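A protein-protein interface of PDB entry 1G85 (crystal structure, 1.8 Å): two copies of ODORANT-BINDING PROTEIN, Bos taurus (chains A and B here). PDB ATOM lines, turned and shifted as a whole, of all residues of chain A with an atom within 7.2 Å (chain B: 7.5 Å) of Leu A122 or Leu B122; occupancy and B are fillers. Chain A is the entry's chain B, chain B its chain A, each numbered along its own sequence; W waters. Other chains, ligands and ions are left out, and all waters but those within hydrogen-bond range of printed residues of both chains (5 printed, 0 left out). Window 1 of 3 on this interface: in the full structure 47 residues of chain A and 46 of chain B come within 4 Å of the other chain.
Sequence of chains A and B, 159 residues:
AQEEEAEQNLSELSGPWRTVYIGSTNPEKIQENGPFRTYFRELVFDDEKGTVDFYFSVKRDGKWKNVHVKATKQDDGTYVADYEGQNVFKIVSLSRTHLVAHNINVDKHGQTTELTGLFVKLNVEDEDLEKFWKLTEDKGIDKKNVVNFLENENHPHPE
Of the printed residues of chain B, Val A120 touches Asn B123.
Leu A122 touches just one residue of chain B: Leu B122.
Of the printed residues of chain B, Asn A123 touches Val B120 (3.3 Å).
Thr B97 touches none of the printed residues of chain A.
Lys B121 touches none of the printed residues of chain A.
Of chain A, only Leu A122 comes within 4 Å of Leu B122.
The nearest residue of chain B that does not touch Leu A122 is Arg B18 (4.4 Å).
The nearest residue of chain A that does not touch Leu B122 is Arg A18 (4.3 Å).
The backbone carbonyl oxygen (O) of Pro B16 lies within hydrogen-bond range of the backbone NH (N) of Leu B122 (2.9 Å).
OG1 of Thr B19 is in hydrogen-bond range of N of Phe B40, at 2.9 Å.
ND2 of Asn B123 sits at hydrogen-bond distance from O of Arg B96 (3.4 Å).
N of Arg A18 sits at hydrogen-bond distance from O of Val A120 (2.8 Å).
The guanidinium group (NH2) of Arg A96 is in hydrogen-bond range of the side-chain amide oxygen (OD1) of Asn A123 (3.0 Å).
Thr A19 touches Leu B150, and with the chains exchanged Leu A150 touches Thr B19.
Val A20 touches Leu B150, and with the chains exchanged Leu A150 touches Val B20.
Val A120 touches Asn B123, and with the chains exchanged Asn A123 touches Val B120.
Leu A122 touches its own counterpart, Leu B122.
Positions printed for both chains: 14, 15, 16, 17, 18, 19, 20, 41, 96, 97, 120, 121, 122, 123, 124 and 150.
Of the 8 pairs that touch across the chains among the printed residues, 7 have their exchanged pair printed and touching as well.
Of the 18 printed residues of chain A, 7 touch a printed residue of chain B.
Hydrophobic or aromatic side chains of chain A within 4 Å of the printed part of chain B: Val A120 and Leu A122.
Hydrophobic or aromatic side chains of chain B within 4 Å of the printed part of chain A: Val B120, Leu B122 and Leu B150.
Among the printed residues, 8 pairs touch across the chains.
Among the printed residues, no Asp or Glu carboxylate lies within 4 Å of a Lys or Arg side-chain nitrogen of the other chain.
CD1 of Leu B150 touches O of Thr A19, at 3.6 Å.
Val A20 touches Leu B150 (O to N, 3.98 Å).
Thr A97 touches Glu B125.
Asn B123 touches Val A120 (O to CG2, 3.4 Å).
CD1 of Leu A122 touches CG of Leu B122, 3.7 Å away.
Asn A123 touches Val B120 (O to CG2, 3.3 Å).
Leu A150 touches Thr B19 (N to O, 3.8 Å).
Val B20 touches Leu A150.
Water W3 lies within hydrogen-bond range of OE2 of Glu A153 (2.5 Å), NE of Arg B18 (2.9 Å) and NE of Arg A18 (3.0 Å).
Water W5 lies within hydrogen-bond range of O of Asn B123 (2.6 Å) and OG1 of Thr A97 (3.4 Å).
Water W2 lies within hydrogen-bond range of OE1 of Glu A153 (2.8 Å), O of Phe B40 (2.9 Å) and N of Thr B19 (3.0 Å).
Water W4 bridges the side-chain carboxylate of Glu A153 (2.9 Å) and the backbone carbonyl oxygen of Phe B40 (3.1 Å).
Water W1 bridges OE2 of Glu B125 (2.9 Å) and OG1 of Thr A97 (3.0 Å).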
ATOM      1  N   SER A  14     -22.248 -12.854 -29.575  1.00  0.00           N
ATOM      2  CA  SER A  14     -22.573 -11.587 -28.926  1.00  0.00           C
ATOM      3  C   SER A  14     -23.020 -11.826 -27.488  1.00  0.00           C
ATOM      4  O   SER A  14     -23.647 -12.840 -27.180  1.00  0.00           O
ATOM      5  CB  SER A  14     -23.689 -10.865 -29.685  1.00  0.00           C
ATOM      6  OG  SER A  14     -23.277 -10.525 -30.995  1.00  0.00           O
ATOM      7  N   GLY A  15     -22.700 -10.889 -26.603  1.00  0.00           N
ATOM      8  CA  GLY A  15     -23.098 -11.043 -25.218  1.00  0.00           C
ATOM      9  C   GLY A  15     -22.037 -10.553 -24.252  1.00  0.00           C
ATOM     10  O   GLY A  15     -21.138  -9.806 -24.642  1.00  0.00           O
ATOM     11  N   PRO A  16     -22.113 -10.960 -22.981  1.00  0.00           N
ATOM     12  CA  PRO A  16     -21.114 -10.515 -22.008  1.00  0.00           C
ATOM     13  C   PRO A  16     -19.747 -11.158 -22.212  1.00  0.00           C
ATOM     14  O   PRO A  16     -19.629 -12.375 -22.338  1.00  0.00           O
ATOM     15  CB  PRO A  16     -21.745 -10.889 -20.669  1.00  0.00           C
ATOM     16  CG  PRO A  16     -22.554 -12.106 -21.005  1.00  0.00           C
ATOM     17  CD  PRO A  16     -23.186 -11.730 -22.325  1.00  0.00           C
ATOM     18  N   TRP A  17     -18.722 -10.317 -22.265  1.00  0.00           N
ATOM     19  CA  TRP A  17     -17.347 -10.762 -22.421  1.00  0.00           C
ATOM     20  C   TRP A  17     -16.535 -10.060 -21.342  1.00  0.00           C
ATOM     21  O   TRP A  17     -16.895  -8.960 -20.905  1.00  0.00           O
ATOM     22  CB  TRP A  17     -16.795 -10.381 -23.797  1.00  0.00           C
ATOM     23  CG  TRP A  17     -17.261 -11.263 -24.927  1.00  0.00           C
ATOM     24  CD1 TRP A  17     -18.460 -11.204 -25.579  1.00  0.00           C
ATOM     25  CD2 TRP A  17     -16.520 -12.324 -25.541  1.00  0.00           C
ATOM     26  NE1 TRP A  17     -18.512 -12.164 -26.569  1.00  0.00           N
ATOM     27  CE2 TRP A  17     -17.332 -12.867 -26.564  1.00  0.00           C
ATOM     28  CE3 TRP A  17     -15.248 -12.875 -25.322  1.00  0.00           C
ATOM     29  CZ2 TRP A  17     -16.911 -13.936 -27.374  1.00  0.00           C
ATOM     30  CZ3 TRP A  17     -14.826 -13.938 -26.123  1.00  0.00           C
ATOM     31  CH2 TRP A  17     -15.658 -14.457 -27.138  1.00  0.00           C
ATOM     32  N   ARG A  18     -15.443 -10.690 -20.919  1.00  0.00           N
ATOM     33  CA  ARG A  18     -14.575 -10.130 -19.890  1.00  0.00           C
ATOM     34  C   ARG A  18     -13.112 -10.174 -20.306  1.00  0.00           C
ATOM     35  O   ARG A  18     -12.672 -11.092 -20.996  1.00  0.00           O
ATOM     36  CB  ARG A  18     -14.736 -10.908 -18.578  1.00  0.00           C
ATOM     37  CG  ARG A  18     -16.124 -10.810 -17.964  1.00  0.00           C
ATOM     38  CD  ARG A  18     -16.417  -9.411 -17.447  1.00  0.00           C
ATOM     39  NE  ARG A  18     -17.738  -9.340 -16.824  1.00  0.00           N
ATOM     40  CZ  ARG A  18     -18.861  -8.993 -17.449  1.00  0.00           C
ATOM     41  NH1 ARG A  18     -20.007  -8.974 -16.778  1.00  0.00           N
ATOM     42  NH2 ARG A  18     -18.843  -8.646 -18.727  1.00  0.00           N
ATOM     43  N   THR A  19     -12.358  -9.179 -19.866  1.00  0.00           N
ATOM     44  CA  THR A  19     -10.938  -9.108 -20.173  1.00  0.00           C
ATOM     45  C   THR A  19     -10.169 -10.013 -19.217  1.00  0.00           C
ATOM     46  O   THR A  19     -10.456 -10.037 -18.022  1.00  0.00           O
ATOM     47  CB  THR A  19     -10.408  -7.673 -19.990  1.00  0.00           C
ATOM     48  OG1 THR A  19     -11.214  -6.762 -20.746  1.00  0.00           O
ATOM     49  CG2 THR A  19      -8.960  -7.568 -20.453  1.00  0.00           C
ATOM     50  N   VAL A  20      -9.206 -10.764 -19.742  1.00  0.00           N
ATOM     51  CA  VAL A  20      -8.382 -11.623 -18.896  1.00  0.00           C
ATOM     52  C   VAL A  20      -6.992 -10.989 -18.829  1.00  0.00           C
ATOM     53  O   VAL A  20      -6.526 -10.615 -17.754  1.00  0.00           O
ATOM     54  CB  VAL A  20      -8.294 -13.058 -19.450  1.00  0.00           C
ATOM     55  CG1 VAL A  20      -7.327 -13.898 -18.600  1.00  0.00           C
ATOM     56  CG2 VAL A  20      -9.680 -13.693 -19.434  1.00  0.00           C
ATOM     57  N   ARG A  41     -17.240  -5.320 -21.210  1.00  0.00           N
ATOM     58  CA  ARG A  41     -18.574  -5.546 -20.668  1.00  0.00           C
ATOM     59  C   ARG A  41     -19.344  -6.452 -21.625  1.00  0.00           C
ATOM     60  O   ARG A  41     -19.807  -7.529 -21.240  1.00  0.00           O
ATOM     61  CB  ARG A  41     -19.325  -4.220 -20.533  1.00  0.00           C
ATOM     62  CG  ARG A  41     -18.775  -3.254 -19.459  1.00  0.00           C
ATOM     63  CD  ARG A  41     -19.021  -1.733 -19.884  1.00  0.00           C
ATOM     64  NE  ARG A  41     -20.411  -1.457 -20.256  1.00  0.00           N
ATOM     65  CZ  ARG A  41     -20.792  -0.416 -20.992  1.00  0.00           C
ATOM     66  NH1 ARG A  41     -22.078  -0.240 -21.286  1.00  0.00           N
ATOM     67  NH2 ARG A  41     -19.887   0.449 -21.444  1.00  0.00           N
ATOM     68  N   ARG A  96     -16.556 -20.003 -29.227  1.00  0.00           N
ATOM     69  CA  ARG A  96     -17.686 -19.775 -28.345  1.00  0.00           C
ATOM     70  C   ARG A  96     -17.313 -19.198 -26.984  1.00  0.00           C
ATOM     71  O   ARG A  96     -18.126 -18.530 -26.352  1.00  0.00           O
ATOM     72  CB  ARG A  96     -18.446 -21.093 -28.142  1.00  0.00           C
ATOM     73  CG  ARG A  96     -19.574 -21.010 -27.121  1.00  0.00           C
ATOM     74  CD  ARG A  96     -20.549 -22.175 -27.270  1.00  0.00           C
ATOM     75  NE  ARG A  96     -21.854 -21.821 -26.723  1.00  0.00           N
ATOM     76  CZ  ARG A  96     -22.158 -21.834 -25.430  1.00  0.00           C
ATOM     77  NH1 ARG A  96     -21.250 -22.198 -24.532  1.00  0.00           N
ATOM     78  NH2 ARG A  96     -23.365 -21.454 -25.035  1.00  0.00           N
ATOM     79  N   THR A  97     -16.085 -19.434 -26.536  1.00  0.00           N
ATOM     80  CA  THR A  97     -15.692 -18.952 -25.221  1.00  0.00           C
ATOM     81  C   THR A  97     -14.473 -18.043 -25.112  1.00  0.00           C
ATOM     82  O   THR A  97     -14.234 -17.478 -24.049  1.00  0.00           O
ATOM     83  CB  THR A  97     -15.445 -20.129 -24.276  1.00  0.00           C
ATOM     84  OG1 THR A  97     -14.411 -20.959 -24.822  1.00  0.00           O
ATOM     85  CG2 THR A  97     -16.721 -20.945 -24.096  1.00  0.00           C
ATOM     86  N   VAL A 120     -12.637 -13.597 -22.482  1.00  0.00           N
ATOM     87  CA  VAL A 120     -13.461 -14.783 -22.308  1.00  0.00           C
ATOM     88  C   VAL A 120     -14.936 -14.400 -22.241  1.00  0.00           C
ATOM     89  O   VAL A 120     -15.293 -13.350 -21.707  1.00  0.00           O
ATOM     90  CB  VAL A 120     -13.066 -15.541 -21.010  1.00  0.00           C
ATOM     91  CG1 VAL A 120     -13.277 -14.646 -19.798  1.00  0.00           C
ATOM     92  CG2 VAL A 120     -13.878 -16.821 -20.873  1.00  0.00           C
ATOM     93  N   LYS A 121     -15.791 -15.251 -22.794  1.00  0.00           N
ATOM     94  CA  LYS A 121     -17.215 -14.993 -22.778  1.00  0.00           C
ATOM     95  C   LYS A 121     -17.885 -15.653 -21.582  1.00  0.00           C
ATOM     96  O   LYS A 121     -17.497 -16.744 -21.157  1.00  0.00           O
ATOM     97  CB  LYS A 121     -17.868 -15.505 -24.064  1.00  0.00           C
ATOM     98  CG  LYS A 121     -19.384 -15.235 -24.084  1.00  0.00           C
ATOM     99  CD  LYS A 121     -20.062 -15.773 -25.299  1.00  0.00           C
ATOM    100  CE  LYS A 121     -21.577 -15.456 -25.228  1.00  0.00           C
ATOM    101  NZ  LYS A 121     -22.306 -16.000 -26.397  1.00  0.00           N
ATOM    102  N   LEU A 122     -18.882 -14.972 -21.033  1.00  0.00           N
ATOM    103  CA  LEU A 122     -19.645 -15.502 -19.917  1.00  0.00           C
ATOM    104  C   LEU A 122     -20.860 -16.139 -20.557  1.00  0.00           C
ATOM    105  O   LEU A 122     -21.700 -15.447 -21.127  1.00  0.00           O
ATOM    106  CB  LEU A 122     -20.085 -14.386 -18.970  1.00  0.00           C
ATOM    107  CG  LEU A 122     -19.168 -14.087 -17.783  1.00  0.00           C
ATOM    108  CD1 LEU A 122     -17.785 -13.697 -18.282  1.00  0.00           C
ATOM    109  CD2 LEU A 122     -19.774 -12.974 -16.939  1.00  0.00           C
ATOM    110  N   ASN A 123     -20.937 -17.463 -20.480  1.00  0.00           N
ATOM    111  CA  ASN A 123     -22.046 -18.194 -21.071  1.00  0.00           C
ATOM    112  C   ASN A 123     -23.057 -18.689 -20.055  1.00  0.00           C
ATOM    113  O   ASN A 123     -22.706 -19.377 -19.096  1.00  0.00           O
ATOM    114  CB  ASN A 123     -21.525 -19.389 -21.870  1.00  0.00           C
ATOM    115  CG  ASN A 123     -21.441 -19.105 -23.352  1.00  0.00           C
ATOM    116  OD1 ASN A 123     -22.452 -18.826 -23.998  1.00  0.00           O
ATOM    117  ND2 ASN A 123     -20.237 -19.176 -23.900  1.00  0.00           N
ATOM    118  N   VAL A 124     -24.315 -18.330 -20.280  1.00  0.00           N
ATOM    119  CA  VAL A 124     -25.409 -18.755 -19.421  1.00  0.00           C
ATOM    120  C   VAL A 124     -26.317 -19.628 -20.281  1.00  0.00           C
ATOM    121  O   VAL A 124     -26.957 -19.142 -21.215  1.00  0.00           O
ATOM    122  CB  VAL A 124     -26.199 -17.546 -18.871  1.00  0.00           C
ATOM    123  CG1 VAL A 124     -25.327 -16.762 -17.902  1.00  0.00           C
ATOM    124  CG2 VAL A 124     -26.643 -16.642 -20.011  1.00  0.00           C
ATOM    125  N   LEU A 150     -25.702  -9.841 -13.408  1.00  0.00           N
ATOM    126  CA  LEU A 150     -24.956  -9.802 -14.656  1.00  0.00           C
ATOM    127  C   LEU A 150     -25.204  -8.525 -15.452  1.00  0.00           C
ATOM    128  O   LEU A 150     -24.264  -7.929 -15.984  1.00  0.00           O
ATOM    129  CB  LEU A 150     -25.288 -11.036 -15.499  1.00  0.00           C
ATOM    130  CG  LEU A 150     -24.616 -11.162 -16.869  1.00  0.00           C
ATOM    131  CD1 LEU A 150     -23.099 -11.073 -16.726  1.00  0.00           C
ATOM    132  CD2 LEU A 150     -25.018 -12.488 -17.490  1.00  0.00           C
ATOM    133  N   GLU A 153     -23.350  -5.564 -13.844  1.00  0.00           N
ATOM    134  CA  GLU A 153     -21.931  -5.540 -14.185  1.00  0.00           C
ATOM    135  C   GLU A 153     -21.721  -5.112 -15.639  1.00  0.00           C
ATOM    136  O   GLU A 153     -20.716  -4.483 -15.956  1.00  0.00           O
ATOM    137  CB  GLU A 153     -21.281  -6.908 -13.959  1.00  0.00           C
ATOM    138  CG  GLU A 153     -21.089  -7.287 -12.475  1.00  0.00           C
ATOM    139  CD  GLU A 153     -20.141  -8.458 -12.301  1.00  0.00           C
ATOM    140  OE1 GLU A 153     -19.978  -8.945 -11.165  1.00  0.00           O
ATOM    141  OE2 GLU A 153     -19.553  -8.890 -13.311  1.00  0.00           O
ATOM    142  N   ASN A 154     -22.667  -5.451 -16.518  1.00  0.00           N
ATOM    143  CA  ASN A 154     -22.563  -5.086 -17.939  1.00  0.00           C
ATOM    144  C   ASN A 154     -22.876  -3.619 -18.189  1.00  0.00           C
ATOM    145  O   ASN A 154     -22.578  -3.088 -19.258  1.00  0.00           O
ATOM    146  CB  ASN A 154     -23.500  -5.945 -18.804  1.00  0.00           C
ATOM    147  CG  ASN A 154     -22.967  -7.349 -19.041  1.00  0.00           C
ATOM    148  OD1 ASN A 154     -23.621  -8.172 -19.684  1.00  0.00           O
ATOM    149  ND2 ASN A 154     -21.782  -7.626 -18.529  1.00  0.00           N
ATOM    150  N   SER B  14     -12.681 -24.921  -8.789  1.00  0.00           N
ATOM    151  CA  SER B  14     -12.141 -23.707  -8.177  1.00  0.00           C
ATOM    152  C   SER B  14     -11.719 -22.712  -9.250  1.00  0.00           C
ATOM    153  O   SER B  14     -11.252 -23.100 -10.326  1.00  0.00           O
ATOM    154  CB  SER B  14     -10.924 -24.035  -7.309  1.00  0.00           C
ATOM    155  OG  SER B  14     -11.245 -24.982  -6.307  1.00  0.00           O
ATOM    156  N   GLY B  15     -11.873 -21.430  -8.947  1.00  0.00           N
ATOM    157  CA  GLY B  15     -11.490 -20.405  -9.892  1.00  0.00           C
ATOM    158  C   GLY B  15     -12.403 -19.201  -9.840  1.00  0.00           C
ATOM    159  O   GLY B  15     -13.152 -19.023  -8.881  1.00  0.00           O
ATOM    160  N   PRO B  16     -12.355 -18.339 -10.863  1.00  0.00           N
ATOM    161  CA  PRO B  16     -13.209 -17.149 -10.888  1.00  0.00           C
ATOM    162  C   PRO B  16     -14.670 -17.471 -11.223  1.00  0.00           C
ATOM    163  O   PRO B  16     -14.959 -18.162 -12.199  1.00  0.00           O
ATOM    164  CB  PRO B  16     -12.531 -16.263 -11.936  1.00  0.00           C
ATOM    165  CG  PRO B  16     -11.942 -17.265 -12.889  1.00  0.00           C
ATOM    166  CD  PRO B  16     -11.388 -18.336 -11.977  1.00  0.00           C
ATOM    167  N   TRP B  17     -15.583 -16.988 -10.386  1.00  0.00           N
ATOM    168  CA  TRP B  17     -17.017 -17.195 -10.586  1.00  0.00           C
ATOM    169  C   TRP B  17     -17.707 -15.843 -10.492  1.00  0.00           C
ATOM    170  O   TRP B  17     -17.199 -14.926  -9.841  1.00  0.00           O
ATOM    171  CB  TRP B  17     -17.610 -18.117  -9.507  1.00  0.00           C
ATOM    172  CG  TRP B  17     -17.256 -19.561  -9.648  1.00  0.00           C
ATOM    173  CD1 TRP B  17     -16.053 -20.146  -9.362  1.00  0.00           C
ATOM    174  CD2 TRP B  17     -18.107 -20.609 -10.125  1.00  0.00           C
ATOM    175  NE1 TRP B  17     -16.104 -21.494  -9.636  1.00  0.00           N
ATOM    176  CE2 TRP B  17     -17.358 -21.806 -10.109  1.00  0.00           C
ATOM    177  CE3 TRP B  17     -19.434 -20.654 -10.577  1.00  0.00           C
ATOM    178  CZ2 TRP B  17     -17.884 -23.036 -10.515  1.00  0.00           C
ATOM    179  CZ3 TRP B  17     -19.963 -21.875 -10.985  1.00  0.00           C
ATOM    180  CH2 TRP B  17     -19.186 -23.048 -10.953  1.00  0.00           C
ATOM    181  N   ARG B  18     -18.867 -15.729 -11.135  1.00  0.00           N
ATOM    182  CA  ARG B  18     -19.633 -14.490 -11.124  1.00  0.00           C
ATOM    183  C   ARG B  18     -21.099 -14.759 -10.818  1.00  0.00           C
ATOM    184  O   ARG B  18     -21.641 -15.804 -11.167  1.00  0.00           O
ATOM    185  CB  ARG B  18     -19.527 -13.776 -12.482  1.00  0.00           C
ATOM    186  CG  ARG B  18     -18.114 -13.318 -12.864  1.00  0.00           C
ATOM    187  CD  ARG B  18     -17.627 -12.169 -11.978  1.00  0.00           C
ATOM    188  NE  ARG B  18     -16.295 -11.710 -12.364  1.00  0.00           N
ATOM    189  CZ  ARG B  18     -15.153 -12.243 -11.939  1.00  0.00           C
ATOM    190  NH1 ARG B  18     -15.159 -13.268 -11.096  1.00  0.00           N
ATOM    191  NH2 ARG B  18     -13.996 -11.744 -12.358  1.00  0.00           N
ATOM    192  N   THR B  19     -21.740 -13.800 -10.161  1.00  0.00           N
ATOM    193  CA  THR B  19     -23.149 -13.914  -9.829  1.00  0.00           C
ATOM    194  C   THR B  19     -23.997 -13.534 -11.035  1.00  0.00           C
ATOM    195  O   THR B  19     -23.716 -12.532 -11.700  1.00  0.00           O
ATOM    196  CB  THR B  19     -23.514 -12.950  -8.690  1.00  0.00           C
ATOM    197  OG1 THR B  19     -22.615 -13.166  -7.599  1.00  0.00           O
ATOM    198  CG2 THR B  19     -24.962 -13.182  -8.218  1.00  0.00           C
ATOM    199  N   VAL B  20     -25.022 -14.333 -11.322  1.00  0.00           N
ATOM    200  CA  VAL B  20     -25.932 -14.028 -12.424  1.00  0.00           C
ATOM    201  C   VAL B  20     -27.248 -13.551 -11.806  1.00  0.00           C
ATOM    202  O   VAL B  20     -27.695 -12.441 -12.072  1.00  0.00           O
ATOM    203  CB  VAL B  20     -26.207 -15.257 -13.307  1.00  0.00           C
ATOM    204  CG1 VAL B  20     -27.174 -14.877 -14.424  1.00  0.00           C
ATOM    205  CG2 VAL B  20     -24.891 -15.789 -13.889  1.00  0.00           C
ATOM    206  N   PHE B  40     -20.021 -12.234  -6.662  1.00  0.00           N
ATOM    207  CA  PHE B  40     -18.965 -13.231  -6.534  1.00  0.00           C
ATOM    208  C   PHE B  40     -17.725 -12.899  -7.358  1.00  0.00           C
ATOM    209  O   PHE B  40     -17.817 -12.290  -8.428  1.00  0.00           O
ATOM    210  CB  PHE B  40     -19.496 -14.604  -6.948  1.00  0.00           C
ATOM    211  CG  PHE B  40     -20.213 -15.343  -5.845  1.00  0.00           C
ATOM    212  CD1 PHE B  40     -20.927 -14.650  -4.868  1.00  0.00           C
ATOM    213  CD2 PHE B  40     -20.184 -16.737  -5.794  1.00  0.00           C
ATOM    214  CE1 PHE B  40     -21.612 -15.337  -3.865  1.00  0.00           C
ATOM    215  CE2 PHE B  40     -20.868 -17.433  -4.794  1.00  0.00           C
ATOM    216  CZ  PHE B  40     -21.575 -16.733  -3.826  1.00  0.00           C
ATOM    217  N   ARG B  41     -16.569 -13.303  -6.843  1.00  0.00           N
ATOM    218  CA  ARG B  41     -15.301 -13.087  -7.524  1.00  0.00           C
ATOM    219  C   ARG B  41     -14.574 -14.416  -7.694  1.00  0.00           C
ATOM    220  O   ARG B  41     -14.098 -14.737  -8.781  1.00  0.00           O
ATOM    221  CB  ARG B  41     -14.397 -12.143  -6.726  1.00  0.00           C
ATOM    222  CG  ARG B  41     -14.948 -10.736  -6.492  1.00  0.00           C
ATOM    223  CD  ARG B  41     -13.803  -9.789  -6.018  1.00  0.00           C
ATOM    224  NE  ARG B  41     -13.073 -10.326  -4.870  1.00  0.00           N
ATOM    225  CZ  ARG B  41     -13.443 -10.167  -3.603  1.00  0.00           C
ATOM    226  NH1 ARG B  41     -12.721 -10.697  -2.625  1.00  0.00           N
ATOM    227  NH2 ARG B  41     -14.525  -9.461  -3.311  1.00  0.00           N
ATOM    228  N   ARG B  96     -19.199 -27.886 -14.673  1.00  0.00           N
ATOM    229  CA  ARG B  96     -17.965 -27.152 -14.915  1.00  0.00           C
ATOM    230  C   ARG B  96     -18.220 -25.676 -15.196  1.00  0.00           C
ATOM    231  O   ARG B  96     -17.311 -24.855 -15.095  1.00  0.00           O
ATOM    232  CB  ARG B  96     -17.209 -27.767 -16.097  1.00  0.00           C
ATOM    233  CG  ARG B  96     -16.495 -29.106 -15.791  1.00  0.00           C
ATOM    234  CD  ARG B  96     -17.443 -30.149 -15.198  1.00  0.00           C
ATOM    235  NE  ARG B  96     -17.089 -30.469 -13.819  1.00  0.00           N
ATOM    236  CZ  ARG B  96     -17.762 -31.318 -13.048  1.00  0.00           C
ATOM    237  NH1 ARG B  96     -18.835 -31.941 -13.519  1.00  0.00           N
ATOM    238  NH2 ARG B  96     -17.360 -31.548 -11.806  1.00  0.00           N
ATOM    239  N   THR B  97     -19.459 -25.335 -15.535  1.00  0.00           N
ATOM    240  CA  THR B  97     -19.785 -23.955 -15.856  1.00  0.00           C
ATOM    241  C   THR B  97     -20.808 -23.226 -14.996  1.00  0.00           C
ATOM    242  O   THR B  97     -20.851 -21.995 -15.010  1.00  0.00           O
ATOM    243  CB  THR B  97     -20.264 -23.855 -17.305  1.00  0.00           C
ATOM    244  OG1 THR B  97     -21.486 -24.590 -17.452  1.00  0.00           O
ATOM    245  CG2 THR B  97     -19.219 -24.427 -18.245  1.00  0.00           C
ATOM    246  N   VAL B 120     -22.035 -18.383 -12.513  1.00  0.00           N
ATOM    247  CA  VAL B 120     -21.356 -18.954 -13.668  1.00  0.00           C
ATOM    248  C   VAL B 120     -19.844 -18.848 -13.508  1.00  0.00           C
ATOM    249  O   VAL B 120     -19.334 -17.892 -12.925  1.00  0.00           O
ATOM    250  CB  VAL B 120     -21.799 -18.248 -14.981  1.00  0.00           C
ATOM    251  CG1 VAL B 120     -21.424 -16.778 -14.946  1.00  0.00           C
ATOM    252  CG2 VAL B 120     -21.160 -18.928 -16.177  1.00  0.00           C
ATOM    253  N   LYS B 121     -19.121 -19.838 -14.017  1.00  0.00           N
ATOM    254  CA  LYS B 121     -17.673 -19.818 -13.898  1.00  0.00           C
ATOM    255  C   LYS B 121     -17.013 -19.217 -15.131  1.00  0.00           C
ATOM    256  O   LYS B 121     -17.490 -19.395 -16.249  1.00  0.00           O
ATOM    257  CB  LYS B 121     -17.131 -21.236 -13.672  1.00  0.00           C
ATOM    258  CG  LYS B 121     -15.604 -21.275 -13.494  1.00  0.00           C
ATOM    259  CD  LYS B 121     -15.063 -22.685 -13.244  1.00  0.00           C
ATOM    260  CE  LYS B 121     -13.521 -22.641 -13.082  1.00  0.00           C
ATOM    261  NZ  LYS B 121     -12.909 -23.969 -12.814  1.00  0.00           N
ATOM    262  N   LEU B 122     -15.933 -18.479 -14.913  1.00  0.00           N
ATOM    263  CA  LEU B 122     -15.184 -17.894 -16.015  1.00  0.00           C
ATOM    264  C   LEU B 122     -14.030 -18.842 -16.281  1.00  0.00           C
ATOM    265  O   LEU B 122     -13.001 -18.782 -15.617  1.00  0.00           O
ATOM    266  CB  LEU B 122     -14.650 -16.512 -15.654  1.00  0.00           C
ATOM    267  CG  LEU B 122     -15.678 -15.386 -15.722  1.00  0.00           C
ATOM    268  CD1 LEU B 122     -16.793 -15.656 -14.728  1.00  0.00           C
ATOM    269  CD2 LEU B 122     -15.002 -14.056 -15.439  1.00  0.00           C
ATOM    270  N   ASN B 123     -14.221 -19.722 -17.254  1.00  0.00           N
ATOM    271  CA  ASN B 123     -13.215 -20.710 -17.605  1.00  0.00           C
ATOM    272  C   ASN B 123     -12.187 -20.194 -18.602  1.00  0.00           C
ATOM    273  O   ASN B 123     -12.540 -19.717 -19.677  1.00  0.00           O
ATOM    274  CB  ASN B 123     -13.896 -21.957 -18.176  1.00  0.00           C
ATOM    275  CG  ASN B 123     -14.786 -22.646 -17.165  1.00  0.00           C
ATOM    276  OD1 ASN B 123     -14.327 -23.043 -16.096  1.00  0.00           O
ATOM    277  ND2 ASN B 123     -16.064 -22.796 -17.497  1.00  0.00           N
ATOM    278  N   VAL B 124     -10.915 -20.283 -18.229  1.00  0.00           N
ATOM    279  CA  VAL B 124      -9.831 -19.859 -19.108  1.00  0.00           C
ATOM    280  C   VAL B 124      -9.071 -21.130 -19.467  1.00  0.00           C
ATOM    281  O   VAL B 124      -8.421 -21.737 -18.613  1.00  0.00           O
ATOM    282  CB  VAL B 124      -8.873 -18.868 -18.410  1.00  0.00           C
ATOM    283  CG1 VAL B 124      -7.787 -18.426 -19.384  1.00  0.00           C
ATOM    284  CG2 VAL B 124      -9.647 -17.660 -17.908  1.00  0.00           C
ATOM    285  N   GLU B 125      -9.173 -21.535 -20.727  1.00  0.00           N
ATOM    286  CA  GLU B 125      -8.524 -22.751 -21.208  1.00  0.00           C
ATOM    287  C   GLU B 125      -7.028 -22.617 -21.474  1.00  0.00           C
ATOM    288  O   GLU B 125      -6.551 -21.560 -21.895  1.00  0.00           O
ATOM    289  CB  GLU B 125      -9.201 -23.231 -22.487  1.00  0.00           C
ATOM    290  CG  GLU B 125     -10.610 -23.699 -22.314  1.00  0.00           C
ATOM    291  CD  GLU B 125     -11.132 -24.350 -23.571  1.00  0.00           C
ATOM    292  OE1 GLU B 125     -10.414 -25.209 -24.122  1.00  0.00           O
ATOM    293  OE2 GLU B 125     -12.250 -24.009 -24.007  1.00  0.00           O
ATOM    294  N   LEU B 150      -8.401 -10.288 -14.264  1.00  0.00           N
ATOM    295  CA  LEU B 150      -9.272 -11.182 -13.511  1.00  0.00           C
ATOM    296  C   LEU B 150      -9.048 -10.997 -12.017  1.00  0.00           C
ATOM    297  O   LEU B 150     -10.000 -10.974 -11.234  1.00  0.00           O
ATOM    298  CB  LEU B 150      -9.012 -12.632 -13.920  1.00  0.00           C
ATOM    299  CG  LEU B 150     -10.208 -13.396 -14.502  1.00  0.00           C
ATOM    300  CD1 LEU B 150     -10.958 -12.534 -15.505  1.00  0.00           C
ATOM    301  CD2 LEU B 150      -9.718 -14.679 -15.148  1.00  0.00           C
HETATM  302  O   HOH W   1     -11.862 -21.947 -26.015  1.00  0.00           O
HETATM  303  O   HOH W   2     -20.295 -11.267  -9.623  1.00  0.00           O
HETATM  304  O   HOH W   3     -17.170  -9.387 -13.867  1.00  0.00           O
HETATM  305  O   HOH W   4     -17.527  -9.576  -9.851  1.00  0.00           O
HETATM  306  O   HOH W   5     -14.293 -20.413 -21.502  1.00  0.00           O
